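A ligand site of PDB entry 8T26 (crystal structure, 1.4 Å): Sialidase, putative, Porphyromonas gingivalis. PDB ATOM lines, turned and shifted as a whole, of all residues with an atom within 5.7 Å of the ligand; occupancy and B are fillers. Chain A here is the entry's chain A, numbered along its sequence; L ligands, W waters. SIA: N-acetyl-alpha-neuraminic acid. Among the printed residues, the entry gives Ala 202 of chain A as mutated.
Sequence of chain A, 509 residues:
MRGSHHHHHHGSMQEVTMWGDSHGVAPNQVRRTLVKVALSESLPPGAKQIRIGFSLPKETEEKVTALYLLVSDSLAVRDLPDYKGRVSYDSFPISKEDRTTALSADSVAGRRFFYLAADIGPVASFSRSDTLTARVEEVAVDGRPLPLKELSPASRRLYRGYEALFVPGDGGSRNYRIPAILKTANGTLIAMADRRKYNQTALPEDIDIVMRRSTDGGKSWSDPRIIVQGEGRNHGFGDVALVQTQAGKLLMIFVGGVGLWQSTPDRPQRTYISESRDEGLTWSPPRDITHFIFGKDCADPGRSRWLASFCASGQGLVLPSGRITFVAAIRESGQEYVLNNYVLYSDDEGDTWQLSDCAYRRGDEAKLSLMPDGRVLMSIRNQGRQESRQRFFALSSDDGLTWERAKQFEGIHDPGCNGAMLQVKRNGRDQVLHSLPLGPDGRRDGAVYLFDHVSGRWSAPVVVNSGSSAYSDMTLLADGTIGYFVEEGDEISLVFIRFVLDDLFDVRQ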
ATOM      1  N   ARG A 177      22.462  -8.910  -8.758  1.00  0.00           N
ATOM      2  CA  ARG A 177      23.438  -7.814  -8.743  1.00  0.00           C
ATOM      3  C   ARG A 177      22.688  -6.514  -8.505  1.00  0.00           C
ATOM      4  O   ARG A 177      21.457  -6.469  -8.546  1.00  0.00           O
ATOM      5  CB  ARG A 177      24.220  -7.722 -10.073  1.00  0.00           C
ATOM      6  CG  ARG A 177      25.460  -8.648 -10.160  1.00  0.00           C
ATOM      7  CD  ARG A 177      26.537  -8.028 -11.081  1.00  0.00           C
ATOM      8  NE  ARG A 177      27.097  -6.849 -10.416  1.00  0.00           N
ATOM      9  CZ  ARG A 177      27.723  -5.867 -11.041  1.00  0.00           C
ATOM     10  NH1 ARG A 177      27.996  -5.940 -12.338  1.00  0.00           N
ATOM     11  NH2 ARG A 177      28.127  -4.805 -10.350  1.00  0.00           N
ATOM     12  N   ILE A 178      23.444  -5.451  -8.228  1.00  0.00           N
ATOM     13  CA  ILE A 178      22.984  -4.056  -8.328  1.00  0.00           C
ATOM     14  C   ILE A 178      22.057  -3.705  -7.161  1.00  0.00           C
ATOM     15  O   ILE A 178      20.860  -3.552  -7.314  1.00  0.00           O
ATOM     16  CB  ILE A 178      22.335  -3.702  -9.686  1.00  0.00           C
ATOM     17  CG1 ILE A 178      23.085  -4.320 -10.866  1.00  0.00           C
ATOM     18  CG2 ILE A 178      22.352  -2.179  -9.784  1.00  0.00           C
ATOM     19  CD1 ILE A 178      24.590  -3.923 -10.951  1.00  0.00           C
ATOM     20  N   ASP A 194      18.739  -6.163  -9.129  1.00  0.00           N
ATOM     21  CA  ASP A 194      18.543  -6.885 -10.386  1.00  0.00           C
ATOM     22  C   ASP A 194      18.463  -8.387 -10.084  1.00  0.00           C
ATOM     23  O   ASP A 194      19.382  -8.967  -9.484  1.00  0.00           O
ATOM     24  CB  ASP A 194      19.777  -6.734 -11.279  1.00  0.00           C
ATOM     25  CG  ASP A 194      19.848  -5.446 -12.069  1.00  0.00           C
ATOM     26  OD1 ASP A 194      19.340  -4.395 -11.683  1.00  0.00           O
ATOM     27  OD2 ASP A 194      20.514  -5.516 -13.126  1.00  0.00           O
ATOM     28  N   ARG A 196      19.069 -11.262 -11.827  1.00  0.00           N
ATOM     29  CA  ARG A 196      19.816 -11.637 -13.028  1.00  0.00           C
ATOM     30  C   ARG A 196      19.634 -13.136 -13.242  1.00  0.00           C
ATOM     31  O   ARG A 196      20.456 -13.985 -12.877  1.00  0.00           O
ATOM     32  CB  ARG A 196      21.274 -11.173 -12.898  1.00  0.00           C
ATOM     33  CG  ARG A 196      21.355  -9.622 -12.857  1.00  0.00           C
ATOM     34  CD  ARG A 196      22.666  -9.078 -13.372  1.00  0.00           C
ATOM     35  NE  ARG A 196      22.571  -7.622 -13.504  1.00  0.00           N
ATOM     36  CZ  ARG A 196      23.565  -6.827 -13.909  1.00  0.00           C
ATOM     37  NH1 ARG A 196      24.764  -7.311 -14.200  1.00  0.00           N
ATOM     38  NH2 ARG A 196      23.329  -5.527 -14.041  1.00  0.00           N
ATOM     39  N   ALA A 202      24.828  -7.781 -17.790  1.00  0.00           N
ATOM     40  CA  ALA A 202      23.999  -6.599 -17.798  1.00  0.00           C
ATOM     41  C   ALA A 202      22.951  -6.637 -18.904  1.00  0.00           C
ATOM     42  O   ALA A 202      22.963  -7.499 -19.778  1.00  0.00           O
ATOM     43  CB  ALA A 202      24.888  -5.368 -18.044  1.00  0.00           C
ATOM     44  N   LEU A 203      22.069  -5.637 -18.893  1.00  0.00           N
ATOM     45  CA  LEU A 203      21.240  -5.421 -20.064  1.00  0.00           C
ATOM     46  C   LEU A 203      22.157  -5.315 -21.292  1.00  0.00           C
ATOM     47  O   LEU A 203      23.233  -4.703 -21.198  1.00  0.00           O
ATOM     48  CB  LEU A 203      20.493  -4.097 -19.883  1.00  0.00           C
ATOM     49  CG  LEU A 203      19.503  -3.985 -18.716  1.00  0.00           C
ATOM     50  CD1 LEU A 203      19.023  -2.570 -18.522  1.00  0.00           C
ATOM     51  CD2 LEU A 203      18.301  -4.940 -18.958  1.00  0.00           C
ATOM     52  N   ASP A 239      18.972  -1.783 -12.730  1.00  0.00           N
ATOM     53  CA  ASP A 239      19.682  -0.582 -12.249  1.00  0.00           C
ATOM     54  C   ASP A 239      18.727   0.375 -11.531  1.00  0.00           C
ATOM     55  O   ASP A 239      18.490   1.497 -11.953  1.00  0.00           O
ATOM     56  CB  ASP A 239      20.452   0.135 -13.379  1.00  0.00           C
ATOM     57  CG  ASP A 239      21.867  -0.445 -13.612  1.00  0.00           C
ATOM     58  OD1 ASP A 239      22.009  -1.664 -13.650  1.00  0.00           O
ATOM     59  OD2 ASP A 239      22.845   0.331 -13.759  1.00  0.00           O
ATOM     60  N   VAL A 255      16.235   1.522 -15.653  1.00  0.00           N
ATOM     61  CA  VAL A 255      16.278   1.438 -17.118  1.00  0.00           C
ATOM     62  C   VAL A 255      15.742   0.111 -17.608  1.00  0.00           C
ATOM     63  O   VAL A 255      15.614  -0.854 -16.856  1.00  0.00           O
ATOM     64  CB  VAL A 255      17.693   1.687 -17.678  1.00  0.00           C
ATOM     65  CG1 VAL A 255      18.071   3.161 -17.551  1.00  0.00           C
ATOM     66  CG2 VAL A 255      18.745   0.798 -17.008  1.00  0.00           C
ATOM     67  N   LEU A 260      23.369  -0.230 -22.606  1.00  0.00           N
ATOM     68  CA  LEU A 260      23.721   1.188 -22.596  1.00  0.00           C
ATOM     69  C   LEU A 260      24.409   1.646 -23.884  1.00  0.00           C
ATOM     70  O   LEU A 260      24.055   2.674 -24.458  1.00  0.00           O
ATOM     71  CB  LEU A 260      24.635   1.420 -21.391  1.00  0.00           C
ATOM     72  CG  LEU A 260      25.178   2.836 -21.244  1.00  0.00           C
ATOM     73  CD1 LEU A 260      24.092   3.838 -20.939  1.00  0.00           C
ATOM     74  CD2 LEU A 260      26.252   2.828 -20.113  1.00  0.00           C
ATOM     75  N   TRP A 261      25.385   0.863 -24.367  1.00  0.00           N
ATOM     76  CA  TRP A 261      26.120   1.274 -25.559  1.00  0.00           C
ATOM     77  C   TRP A 261      25.389   0.942 -26.857  1.00  0.00           C
ATOM     78  O   TRP A 261      25.862   1.385 -27.911  1.00  0.00           O
ATOM     79  CB  TRP A 261      27.519   0.652 -25.542  1.00  0.00           C
ATOM     80  CG  TRP A 261      28.234   1.008 -24.269  1.00  0.00           C
ATOM     81  CD1 TRP A 261      28.565   0.152 -23.245  1.00  0.00           C
ATOM     82  CD2 TRP A 261      28.666   2.321 -23.853  1.00  0.00           C
ATOM     83  NE1 TRP A 261      29.184   0.850 -22.228  1.00  0.00           N
ATOM     84  CE2 TRP A 261      29.264   2.174 -22.579  1.00  0.00           C
ATOM     85  CE3 TRP A 261      28.595   3.586 -24.436  1.00  0.00           C
ATOM     86  CZ2 TRP A 261      29.824   3.271 -21.881  1.00  0.00           C
ATOM     87  CZ3 TRP A 261      29.144   4.683 -23.748  1.00  0.00           C
ATOM     88  CH2 TRP A 261      29.741   4.502 -22.461  1.00  0.00           C
ATOM     89  N   GLN A 269      17.534   2.638 -24.945  1.00  0.00           N
ATOM     90  CA  GLN A 269      17.367   2.039 -23.625  1.00  0.00           C
ATOM     91  C   GLN A 269      16.645   3.076 -22.766  1.00  0.00           C
ATOM     92  O   GLN A 269      17.126   4.206 -22.599  1.00  0.00           O
ATOM     93  CB  GLN A 269      18.748   1.721 -23.052  1.00  0.00           C
ATOM     94  CG  GLN A 269      18.689   1.249 -21.602  1.00  0.00           C
ATOM     95  CD  GLN A 269      20.059   1.270 -20.940  1.00  0.00           C
ATOM     96  OE1 GLN A 269      20.539   2.313 -20.508  1.00  0.00           O
ATOM     97  NE2 GLN A 269      20.684   0.095 -20.803  1.00  0.00           N
ATOM     98  N   PHE A 310      21.459   6.717 -18.090  1.00  0.00           N
ATOM     99  CA  PHE A 310      20.970   5.884 -16.980  1.00  0.00           C
ATOM    100  C   PHE A 310      21.304   6.588 -15.686  1.00  0.00           C
ATOM    101  O   PHE A 310      22.363   7.199 -15.574  1.00  0.00           O
ATOM    102  CB  PHE A 310      21.508   4.426 -16.995  1.00  0.00           C
ATOM    103  CG  PHE A 310      22.953   4.242 -16.599  1.00  0.00           C
ATOM    104  CD1 PHE A 310      23.989   4.775 -17.357  1.00  0.00           C
ATOM    105  CD2 PHE A 310      23.292   3.476 -15.439  1.00  0.00           C
ATOM    106  CE1 PHE A 310      25.321   4.571 -17.016  1.00  0.00           C
ATOM    107  CE2 PHE A 310      24.629   3.225 -15.091  1.00  0.00           C
ATOM    108  CZ  PHE A 310      25.661   3.799 -15.878  1.00  0.00           C
ATOM    109  N   LEU A 339      30.580   9.211 -21.297  1.00  0.00           N
ATOM    110  CA  LEU A 339      29.340   9.710 -20.753  1.00  0.00           C
ATOM    111  C   LEU A 339      29.583  11.031 -20.039  1.00  0.00           C
ATOM    112  O   LEU A 339      30.666  11.269 -19.528  1.00  0.00           O
ATOM    113  CB  LEU A 339      28.786   8.731 -19.684  1.00  0.00           C
ATOM    114  CG  LEU A 339      28.581   7.284 -20.155  1.00  0.00           C
ATOM    115  CD1 LEU A 339      28.238   6.346 -18.973  1.00  0.00           C
ATOM    116  CD2 LEU A 339      27.442   7.229 -21.173  1.00  0.00           C
ATOM    117  N   ASP A 364      30.511   9.015 -15.049  1.00  0.00           N
ATOM    118  CA  ASP A 364      29.896   7.684 -15.035  1.00  0.00           C
ATOM    119  C   ASP A 364      28.937   7.722 -13.848  1.00  0.00           C
ATOM    120  O   ASP A 364      28.516   8.816 -13.442  1.00  0.00           O
ATOM    121  CB  ASP A 364      30.959   6.591 -14.928  1.00  0.00           C
ATOM    122  CG  ASP A 364      30.490   5.268 -15.490  1.00  0.00           C
ATOM    123  OD1 ASP A 364      29.695   4.579 -14.813  1.00  0.00           O
ATOM    124  OD2 ASP A 364      30.844   4.918 -16.662  1.00  0.00           O
ATOM    125  N   GLU A 365      28.584   6.567 -13.277  1.00  0.00           N
ATOM    126  CA  GLU A 365      27.619   6.554 -12.166  1.00  0.00           C
ATOM    127  C   GLU A 365      28.000   7.554 -11.084  1.00  0.00           C
ATOM    128  O   GLU A 365      29.106   7.521 -10.562  1.00  0.00           O
ATOM    129  CB  GLU A 365      27.645   5.164 -11.533  1.00  0.00           C
ATOM    130  CG  GLU A 365      27.011   4.080 -12.421  1.00  0.00           C
ATOM    131  CD  GLU A 365      27.398   2.697 -11.982  1.00  0.00           C
ATOM    132  OE1 GLU A 365      28.453   2.577 -11.308  1.00  0.00           O
ATOM    133  OE2 GLU A 365      26.679   1.718 -12.341  1.00  0.00           O
ATOM    134  N   ARG A 381      31.925   8.209 -10.316  1.00  0.00           N
ATOM    135  CA  ARG A 381      32.780   7.071 -10.598  1.00  0.00           C
ATOM    136  C   ARG A 381      33.797   7.426 -11.678  1.00  0.00           C
ATOM    137  O   ARG A 381      33.469   8.028 -12.710  1.00  0.00           O
ATOM    138  CB  ARG A 381      31.911   5.880 -11.042  1.00  0.00           C
ATOM    139  CG  ARG A 381      32.610   4.729 -11.801  1.00  0.00           C
ATOM    140  CD  ARG A 381      31.588   3.621 -12.059  1.00  0.00           C
ATOM    141  NE  ARG A 381      32.107   2.599 -12.948  1.00  0.00           N
ATOM    142  CZ  ARG A 381      31.515   1.425 -13.141  1.00  0.00           C
ATOM    143  NH1 ARG A 381      30.427   1.065 -12.454  1.00  0.00           N
ATOM    144  NH2 ARG A 381      32.007   0.588 -14.067  1.00  0.00           N
ATOM    145  N   GLN A 383      35.618   6.118 -14.591  1.00  0.00           N
ATOM    146  CA  GLN A 383      35.556   5.012 -15.548  1.00  0.00           C
ATOM    147  C   GLN A 383      36.694   5.156 -16.536  1.00  0.00           C
ATOM    148  O   GLN A 383      36.922   6.247 -17.065  1.00  0.00           O
ATOM    149  CB  GLN A 383      34.197   5.011 -16.265  1.00  0.00           C
ATOM    150  CG  GLN A 383      34.007   3.866 -17.259  1.00  0.00           C
ATOM    151  CD  GLN A 383      34.000   2.486 -16.610  1.00  0.00           C
ATOM    152  OE1 GLN A 383      33.788   2.367 -15.407  1.00  0.00           O
ATOM    153  NE2 GLN A 383      34.284   1.436 -17.401  1.00  0.00           N
ATOM    154  N   GLY A 416      36.817   1.962 -10.264  1.00  0.00           N
ATOM    155  CA  GLY A 416      35.816   2.104 -11.309  1.00  0.00           C
ATOM    156  C   GLY A 416      34.559   1.368 -10.912  1.00  0.00           C
ATOM    157  O   GLY A 416      34.231   0.365 -11.540  1.00  0.00           O
ATOM    158  N   ARG A 443      37.890  -5.035  -7.930  1.00  0.00           N
ATOM    159  CA  ARG A 443      36.712  -5.004  -7.069  1.00  0.00           C
ATOM    160  C   ARG A 443      36.942  -5.994  -5.934  1.00  0.00           C
ATOM    161  O   ARG A 443      36.468  -7.140  -5.940  1.00  0.00           O
ATOM    162  CB  ARG A 443      35.458  -5.282  -7.894  1.00  0.00           C
ATOM    163  CG  ARG A 443      34.984  -4.005  -8.625  1.00  0.00           C
ATOM    164  CD  ARG A 443      33.967  -4.286  -9.666  1.00  0.00           C
ATOM    165  NE  ARG A 443      33.703  -3.103 -10.476  1.00  0.00           N
ATOM    166  CZ  ARG A 443      32.585  -2.962 -11.185  1.00  0.00           C
ATOM    167  NH1 ARG A 443      31.639  -3.867 -11.144  1.00  0.00           N
ATOM    168  NH2 ARG A 443      32.438  -1.880 -11.943  1.00  0.00           N
ATOM    169  N   TYR A 471      29.509  -3.227  -6.002  1.00  0.00           N
ATOM    170  CA  TYR A 471      28.642  -2.083  -5.708  1.00  0.00           C
ATOM    171  C   TYR A 471      28.176  -2.108  -4.262  1.00  0.00           C
ATOM    172  O   TYR A 471      27.981  -3.177  -3.645  1.00  0.00           O
ATOM    173  CB  TYR A 471      27.390  -2.157  -6.592  1.00  0.00           C
ATOM    174  CG  TYR A 471      27.576  -1.716  -8.044  1.00  0.00           C
ATOM    175  CD1 TYR A 471      28.831  -1.778  -8.664  1.00  0.00           C
ATOM    176  CD2 TYR A 471      26.492  -1.260  -8.785  1.00  0.00           C
ATOM    177  CE1 TYR A 471      28.991  -1.352  -9.984  1.00  0.00           C
ATOM    178  CE2 TYR A 471      26.628  -0.830 -10.089  1.00  0.00           C
ATOM    179  CZ  TYR A 471      27.889  -0.904 -10.716  1.00  0.00           C
ATOM    180  OH  TYR A 471      28.007  -0.457 -12.001  1.00  0.00           O
ATOM    181  N   GLU A 487      27.639  -5.948  -2.690  1.00  0.00           N
ATOM    182  CA  GLU A 487      27.836  -7.127  -3.540  1.00  0.00           C
ATOM    183  C   GLU A 487      29.078  -7.876  -3.049  1.00  0.00           C
ATOM    184  O   GLU A 487      30.194  -7.456  -3.307  1.00  0.00           O
ATOM    185  CB  GLU A 487      28.069  -6.667  -4.981  1.00  0.00           C
ATOM    186  CG  GLU A 487      26.889  -5.912  -5.582  1.00  0.00           C
ATOM    187  CD  GLU A 487      27.048  -5.737  -7.063  1.00  0.00           C
ATOM    188  OE1 GLU A 487      28.055  -5.137  -7.521  1.00  0.00           O
ATOM    189  OE2 GLU A 487      26.170  -6.180  -7.825  1.00  0.00           O
HETATM  190  C1  SIA L   1      29.288  -2.587 -13.634  1.00  0.00           C
HETATM  191  C2  SIA L   1      28.044  -2.349 -14.491  1.00  0.00           C
HETATM  192  C3  SIA L   1      26.725  -2.626 -13.773  1.00  0.00           C
HETATM  193  C4  SIA L   1      25.526  -1.886 -14.270  1.00  0.00           C
HETATM  194  C5  SIA L   1      25.768  -1.152 -15.569  1.00  0.00           C
HETATM  195  C6  SIA L   1      26.957  -0.219 -15.396  1.00  0.00           C
HETATM  196  C7  SIA L   1      27.315   0.537 -16.654  1.00  0.00           C
HETATM  197  C8  SIA L   1      28.656   1.266 -16.453  1.00  0.00           C
HETATM  198  C9  SIA L   1      28.874   2.195 -17.656  1.00  0.00           C
HETATM  199  C10 SIA L   1      24.027  -0.290 -17.213  1.00  0.00           C
HETATM  200  C11 SIA L   1      22.690   0.415 -17.444  1.00  0.00           C
HETATM  201  N5  SIA L   1      24.509  -0.420 -15.855  1.00  0.00           N
HETATM  202  O1A SIA L   1      29.342  -3.501 -12.768  1.00  0.00           O
HETATM  203  O1B SIA L   1      30.322  -1.877 -13.800  1.00  0.00           O
HETATM  204  O2  SIA L   1      28.137  -3.203 -15.558  1.00  0.00           O
HETATM  205  O4  SIA L   1      24.425  -2.833 -14.446  1.00  0.00           O
HETATM  206  O6  SIA L   1      28.166  -0.966 -15.035  1.00  0.00           O
HETATM  207  O7  SIA L   1      27.444  -0.303 -17.791  1.00  0.00           O
HETATM  208  O8  SIA L   1      28.601   2.015 -15.259  1.00  0.00           O
HETATM  209  O9  SIA L   1      30.226   2.573 -17.712  1.00  0.00           O
HETATM  210  O10 SIA L   1      24.656  -0.710 -18.159  1.00  0.00           O
HETATM  211  O   HOH W   1      31.275  -1.995 -16.440  1.00  0.00           O
HETATM  212  O   HOH W   2      26.735  -5.543 -15.245  1.00  0.00           O
HETATM  213  O   HOH W   3      23.536  -1.880 -20.325  1.00  0.00           O
HETATM  214  O   HOH W   4      22.433  -3.493 -16.885  1.00  0.00           O
HETATM  215  O   HOH W   5      29.886  -0.743 -19.746  1.00  0.00           O
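The side-chain carboxylate of Asp 364 is in hydrogen-bond range of an oxygen (O9) of the ligand, at 2.6 Å.
A nitrogen (N5) of the ligand lies within hydrogen-bond range of the side-chain carboxylate of Asp 239 (2.8 Å).
NH2 of Arg 443 is in salt-bridge range of O1B of the ligand (2.8 Å).
NH1 of Arg 177 lies within salt-bridge range of O1A of the ligand, 2.8 Å away.
NH2 of Arg 196 lies within hydrogen-bond range of O4 of the ligand, 2.9 Å away.
The side-chain hydroxyl (OH) of Tyr 471 sits close to an oxygen (O6) of the ligand (3.1 Å).
O1B of the ligand is in salt-bridge range of NH2 of Arg 381.
Ile 178 touches the ligand.
CG2 of Val 255 touches C11 of the ligand, 3.99 Å away.
CD2 of Leu 260 touches C9 of the ligand, 3.6 Å away.
Gln 269 touches the ligand (NE2 to C11, 3.9 Å).
CZ of Phe 310 touches O8 of the ligand, at 3.5 Å.
Glu 365 touches the ligand.
Gln 383 touches the ligand (CD to O9, 3.9 Å).
Hydrophobic or aromatic side chains that line the ligand: Ile 178, Val 255, Leu 260, Phe 310 and Tyr 471.
Along chain A the residues within 4 Å of the ligand span positions 177 to 471.
The nearest printed residue that does not touch the ligand is Trp 261 (4.2 Å).
Water W3 lies within hydrogen-bond range of an oxygen (O10) of the ligand (2.7 Å), the backbone NH (N) of Leu 260 (2.8 Å) and the backbone carbonyl oxygen (O) of Leu 203 (3.0 Å).
Water W2 lies within hydrogen-bond range of O2 of the ligand (2.7 Å), NH1 of Arg 196 (2.8 Å) and NH1 of Arg 177 (3.2 Å).
Water W5 lies within hydrogen-bond range of the indole nitrogen (NE1) of Trp 261 and an oxygen (O7) of the ligand.
Water W4 lies within hydrogen-bond range of N of Leu 203 (3.0 Å) and O4 of the ligand (3.2 Å).
The side-chain carboxylate (OD1) of Asp 364 is in salt-bridge range of the guanidinium group (NE) of Arg 381, at 3.6 Å.
N of Asp 239 lies within hydrogen-bond range of OD1 of Asp 194 (2.8 Å).
The backbone carbonyl oxygen of Gly 416 lies within hydrogen-bond range of the guanidinium group of Arg 443, 2.9 Å away.
The backbone NH (N) of Asp 194 sits at hydrogen-bond distance from the backbone carbonyl oxygen (O) of Arg 177, 2.8 Å away.
The side-chain carboxylate (OE2) of Glu 487 is in salt-bridge range of the guanidinium group (NE) of Arg 177.
The side-chain carboxylate (OE2) of Glu 365 is in hydrogen-bond range of the side-chain hydroxyl (OH) of Tyr 471, at 2.6 Å.
O of Gly 416 lies close to NH2 of Arg 381, at 3.4 Å.
The backbone NH of Leu 260 lies close to the side-chain amide nitrogen of Gln 269, 3.3 Å away.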
